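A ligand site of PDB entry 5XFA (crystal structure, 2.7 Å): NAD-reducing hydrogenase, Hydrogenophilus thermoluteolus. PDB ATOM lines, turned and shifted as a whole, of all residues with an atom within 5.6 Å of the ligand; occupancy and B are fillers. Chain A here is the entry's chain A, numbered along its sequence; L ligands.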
ATOM      1  N   VAL A 315       4.342   1.588  14.891  1.00  0.00           N
ATOM      2  CA  VAL A 315       5.019   2.884  15.064  1.00  0.00           C
ATOM      3  C   VAL A 315       5.086   3.665  13.748  1.00  0.00           C
ATOM      4  O   VAL A 315       5.039   4.896  13.776  1.00  0.00           O
ATOM      5  CB  VAL A 315       6.420   2.746  15.698  1.00  0.00           C
ATOM      6  CG1 VAL A 315       7.361   1.954  14.791  1.00  0.00           C
ATOM      7  CG2 VAL A 315       6.999   4.112  16.038  1.00  0.00           C
ATOM      8  N   PRO A 333      10.882   7.426  15.093  1.00  0.00           N
ATOM      9  CA  PRO A 333      10.535   8.844  14.988  1.00  0.00           C
ATOM     10  C   PRO A 333      11.752   9.742  15.043  1.00  0.00           C
ATOM     11  O   PRO A 333      12.720   9.463  15.744  1.00  0.00           O
ATOM     12  CB  PRO A 333       9.656   9.063  16.207  1.00  0.00           C
ATOM     13  CG  PRO A 333       8.978   7.748  16.416  1.00  0.00           C
ATOM     14  CD  PRO A 333      10.039   6.731  16.087  1.00  0.00           C
ATOM     15  N   GLU A 477       5.529  -3.159  19.922  1.00  0.00           N
ATOM     16  CA  GLU A 477       5.570  -2.260  18.787  1.00  0.00           C
ATOM     17  C   GLU A 477       6.403  -0.999  19.048  1.00  0.00           C
ATOM     18  O   GLU A 477       6.689  -0.233  18.121  1.00  0.00           O
ATOM     19  CB  GLU A 477       4.139  -1.923  18.361  1.00  0.00           C
ATOM     20  CG  GLU A 477       3.333  -3.146  17.904  1.00  0.00           C
ATOM     21  CD  GLU A 477       3.641  -3.639  16.496  1.00  0.00           C
ATOM     22  OE1 GLU A 477       4.177  -2.861  15.665  1.00  0.00           O
ATOM     23  OE2 GLU A 477       3.349  -4.815  16.190  1.00  0.00           O
ATOM     24  N   SER A 478       6.829  -0.799  20.287  1.00  0.00           N
ATOM     25  CA  SER A 478       7.730   0.304  20.623  1.00  0.00           C
ATOM     26  C   SER A 478       9.002   0.309  19.802  1.00  0.00           C
ATOM     27  O   SER A 478       9.626  -0.724  19.638  1.00  0.00           O
ATOM     28  CB  SER A 478       8.152   0.240  22.091  1.00  0.00           C
ATOM     29  OG  SER A 478       9.089   1.261  22.366  1.00  0.00           O
ATOM     30  N   CYS A 479       9.410   1.488  19.330  1.00  0.00           N
ATOM     31  CA  CYS A 479      10.585   1.550  18.461  1.00  0.00           C
ATOM     32  C   CYS A 479      11.926   1.397  19.208  1.00  0.00           C
ATOM     33  O   CYS A 479      12.945   1.213  18.575  1.00  0.00           O
ATOM     34  CB  CYS A 479      10.575   2.820  17.601  1.00  0.00           C
ATOM     35  SG  CYS A 479      11.480   4.230  18.258  1.00  0.00           S
ATOM     36  N   GLY A 480      11.904   1.472  20.538  1.00  0.00           N
ATOM     37  CA  GLY A 480      13.099   1.188  21.355  1.00  0.00           C
ATOM     38  C   GLY A 480      14.137   2.322  21.381  1.00  0.00           C
ATOM     39  O   GLY A 480      15.266   2.145  21.856  1.00  0.00           O
ATOM     40  N   PHE A 481      13.759   3.486  20.874  1.00  0.00           N
ATOM     41  CA  PHE A 481      14.719   4.579  20.706  1.00  0.00           C
ATOM     42  C   PHE A 481      14.981   5.323  22.027  1.00  0.00           C
ATOM     43  O   PHE A 481      16.097   5.790  22.257  1.00  0.00           O
ATOM     44  CB  PHE A 481      14.258   5.588  19.584  1.00  0.00           C
ATOM     45  CG  PHE A 481      15.083   6.823  19.559  1.00  0.00           C
ATOM     46  CD1 PHE A 481      16.398   6.767  19.155  1.00  0.00           C
ATOM     47  CD2 PHE A 481      14.591   8.012  20.038  1.00  0.00           C
ATOM     48  CE1 PHE A 481      17.220   7.903  19.175  1.00  0.00           C
ATOM     49  CE2 PHE A 481      15.386   9.166  20.062  1.00  0.00           C
ATOM     50  CZ  PHE A 481      16.710   9.113  19.623  1.00  0.00           C
ATOM     51  N   CYS A 482      13.954   5.510  22.849  1.00  0.00           N
ATOM     52  CA  CYS A 482      14.065   6.436  23.992  1.00  0.00           C
ATOM     53  C   CYS A 482      13.753   5.782  25.336  1.00  0.00           C
ATOM     54  O   CYS A 482      12.942   4.876  25.448  1.00  0.00           O
ATOM     55  CB  CYS A 482      13.238   7.732  23.734  1.00  0.00           C
ATOM     56  SG  CYS A 482      11.438   7.762  23.977  1.00  0.00           S
ATOM     57  N   CYS A 485      10.106   4.916  27.152  1.00  0.00           N
ATOM     58  CA  CYS A 485       9.185   4.136  26.347  1.00  0.00           C
ATOM     59  C   CYS A 485       9.766   2.763  26.074  1.00  0.00           C
ATOM     60  O   CYS A 485       9.051   1.778  26.143  1.00  0.00           O
ATOM     61  CB  CYS A 485       8.911   4.867  25.036  1.00  0.00           C
ATOM     62  SG  CYS A 485       7.936   3.864  23.918  1.00  0.00           S
ATOM     63  N   ARG A 486      11.057   2.710  25.760  1.00  0.00           N
ATOM     64  CA  ARG A 486      11.714   1.445  25.449  1.00  0.00           C
ATOM     65  C   ARG A 486      11.565   0.493  26.601  1.00  0.00           C
ATOM     66  O   ARG A 486      11.084  -0.625  26.424  1.00  0.00           O
ATOM     67  CB  ARG A 486      13.209   1.634  25.194  1.00  0.00           C
ATOM     68  CG  ARG A 486      13.997   0.331  25.045  1.00  0.00           C
ATOM     69  CD  ARG A 486      15.404   0.582  24.524  1.00  0.00           C
ATOM     70  NE  ARG A 486      16.279   1.202  25.518  1.00  0.00           N
ATOM     71  CZ  ARG A 486      16.623   2.485  25.584  1.00  0.00           C
ATOM     72  NH1 ARG A 486      16.185   3.394  24.717  1.00  0.00           N
ATOM     73  NH2 ARG A 486      17.424   2.883  26.572  1.00  0.00           N
ATOM     74  N   SER A 523       8.722  10.791  27.183  1.00  0.00           N
ATOM     75  CA  SER A 523       8.826  10.141  25.860  1.00  0.00           C
ATOM     76  C   SER A 523       9.166  11.115  24.733  1.00  0.00           C
ATOM     77  O   SER A 523       8.876  12.289  24.813  1.00  0.00           O
ATOM     78  CB  SER A 523       7.502   9.433  25.492  1.00  0.00           C
ATOM     79  OG  SER A 523       7.406   8.176  26.125  1.00  0.00           O
ATOM     80  N   ASN A 524       9.729  10.587  23.660  1.00  0.00           N
ATOM     81  CA  ASN A 524      10.120  11.417  22.516  1.00  0.00           C
ATOM     82  C   ASN A 524       9.016  11.589  21.469  1.00  0.00           C
ATOM     83  O   ASN A 524       9.027  12.555  20.742  1.00  0.00           O
ATOM     84  CB  ASN A 524      11.377  10.833  21.861  1.00  0.00           C
ATOM     85  CG  ASN A 524      11.670  11.423  20.479  1.00  0.00           C
ATOM     86  OD1 ASN A 524      12.105  12.562  20.347  1.00  0.00           O
ATOM     87  ND2 ASN A 524      11.432  10.643  19.444  1.00  0.00           N
ATOM     88  N   CYS A 525       8.089  10.644  21.389  1.00  0.00           N
ATOM     89  CA  CYS A 525       6.963  10.755  20.479  1.00  0.00           C
ATOM     90  C   CYS A 525       5.620  10.362  21.119  1.00  0.00           C
ATOM     91  O   CYS A 525       5.574   9.953  22.266  1.00  0.00           O
ATOM     92  CB  CYS A 525       7.251   9.931  19.225  1.00  0.00           C
ATOM     93  SG  CYS A 525       6.808   8.196  19.357  1.00  0.00           S
ATOM     94  N   GLY A 526       4.540  10.506  20.373  1.00  0.00           N
ATOM     95  CA  GLY A 526       3.184  10.343  20.900  1.00  0.00           C
ATOM     96  C   GLY A 526       2.782   8.916  21.170  1.00  0.00           C
ATOM     97  O   GLY A 526       1.753   8.679  21.808  1.00  0.00           O
ATOM     98  N   PHE A 527       3.558   7.959  20.677  1.00  0.00           N
ATOM     99  CA  PHE A 527       3.381   6.557  21.009  1.00  0.00           C
ATOM    100  C   PHE A 527       3.702   6.305  22.506  1.00  0.00           C
ATOM    101  O   PHE A 527       2.919   5.688  23.210  1.00  0.00           O
ATOM    102  CB  PHE A 527       4.255   5.702  20.090  1.00  0.00           C
ATOM    103  CG  PHE A 527       4.242   4.229  20.398  1.00  0.00           C
ATOM    104  CD1 PHE A 527       4.827   3.738  21.554  1.00  0.00           C
ATOM    105  CD2 PHE A 527       3.705   3.336  19.485  1.00  0.00           C
ATOM    106  CE1 PHE A 527       4.834   2.380  21.809  1.00  0.00           C
ATOM    107  CE2 PHE A 527       3.720   1.965  19.720  1.00  0.00           C
ATOM    108  CZ  PHE A 527       4.287   1.495  20.891  1.00  0.00           C
ATOM    109  N   GLY A 528       4.852   6.765  22.986  1.00  0.00           N
ATOM    110  CA  GLY A 528       5.208   6.639  24.397  1.00  0.00           C
ATOM    111  C   GLY A 528       4.298   7.396  25.348  1.00  0.00           C
ATOM    112  O   GLY A 528       4.152   7.040  26.514  1.00  0.00           O
ATOM    113  N   LEU A 529       3.675   8.447  24.832  1.00  0.00           N
ATOM    114  CA  LEU A 529       2.699   9.204  25.595  1.00  0.00           C
ATOM    115  C   LEU A 529       1.373   8.414  25.693  1.00  0.00           C
ATOM    116  O   LEU A 529       0.805   8.306  26.768  1.00  0.00           O
ATOM    117  CB  LEU A 529       2.516  10.584  24.953  1.00  0.00           C
ATOM    118  CG  LEU A 529       1.346  11.485  25.428  1.00  0.00           C
ATOM    119  CD1 LEU A 529       1.196  11.449  26.935  1.00  0.00           C
ATOM    120  CD2 LEU A 529       1.463  12.944  24.956  1.00  0.00           C
HETATM  121 FE1  LIG L   1       8.527   4.963  22.045  1.00  0.00          FE
HETATM  122 FE2  LIG L   1      10.488   5.282  20.054  1.00  0.00          FE
HETATM  123 FE3  LIG L   1      10.518   6.650  22.309  1.00  0.00          FE
HETATM  124 FE4  LIG L   1       8.456   6.956  20.429  1.00  0.00          FE
HETATM  125  S1  LIG L   1      10.639   7.501  20.219  1.00  0.00           S
HETATM  126  S2  LIG L   1       8.354   7.095  22.697  1.00  0.00           S
HETATM  127  S3  LIG L   1       8.290   4.761  19.820  1.00  0.00           S
HETATM  128  S4  LIG L   1      10.754   4.414  22.128  1.00  0.00           S
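A sulfur (S2) of the ligand sits close to the backbone NH of Cys 525, 3.8 Å away.
A sulfur (S4) of the ligand lies close to the side-chain hydroxyl (OG) of Ser 478.
An iron atom (FE3) of the ligand is bound by the side-chain sulfur of Cys 482, 2.2 Å away.
FE4 of the ligand is bound by SG of Cys 525 (2.3 Å).
SG of Cys 485 binds FE1 of the ligand.
ND2 of Asn 524 sits close to S1 of the ligand, at 3.3 Å.
FE2 of the ligand is bound by SG of Cys 479, 2.3 Å away.
S2 of the ligand sits close to OG of Ser 523 (3.7 Å).
The backbone NH (N) of Gly 480 sits close to a sulfur (S4) of the ligand (3.5 Å).
The backbone NH of Gly 528 lies close to a sulfur (S2) of the ligand (3.5 Å).
N of Cys 482 sits close to S4 of the ligand (3.5 Å).
S3 of the ligand sits close to N of Cys 479.
S4 of the ligand lies close to N of Phe 481 (3.4 Å).
The backbone carbonyl oxygen of Phe 481 sits at hydrogen-bond distance from the guanidinium group of Arg 486 (3.4 Å).
The side-chain sulfur of Cys 485 lies close to the side-chain hydroxyl of Ser 478.
The side-chain sulfur (SG) of Cys 479 lies close to the backbone NH (N) of Phe 481 (3.5 Å).
N of Asn 524 sits close to SG of Cys 482 (3.3 Å).
N of Gly 480 lies close to OG of Ser 478 (3.4 Å).
The backbone carbonyl oxygen (O) of Gly 528 sits close to the side-chain hydroxyl (OG) of Ser 523, 3.5 Å away.
NH1 of Arg 486 sits close to O of Gly 480 (3.3 Å).
The side-chain sulfur of Cys 525 sits close to the backbone NH of Phe 527 (3.5 Å).
Merely in contact with the ligand: Phe 527 (3.9 Å).
Hydrophobic or aromatic side chains within 4 Å of the ligand: Phe 481 and Phe 527.
11 residues have an atom within 4 Å of the ligand: Ser 478, Cys 479, Gly 480, Phe 481, Cys 482, Cys 485, Ser 523, Asn 524, Cys 525, Phe 527 and Gly 528.
The nearest printed residue that does not touch the ligand is Arg 486 (4.02 Å).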
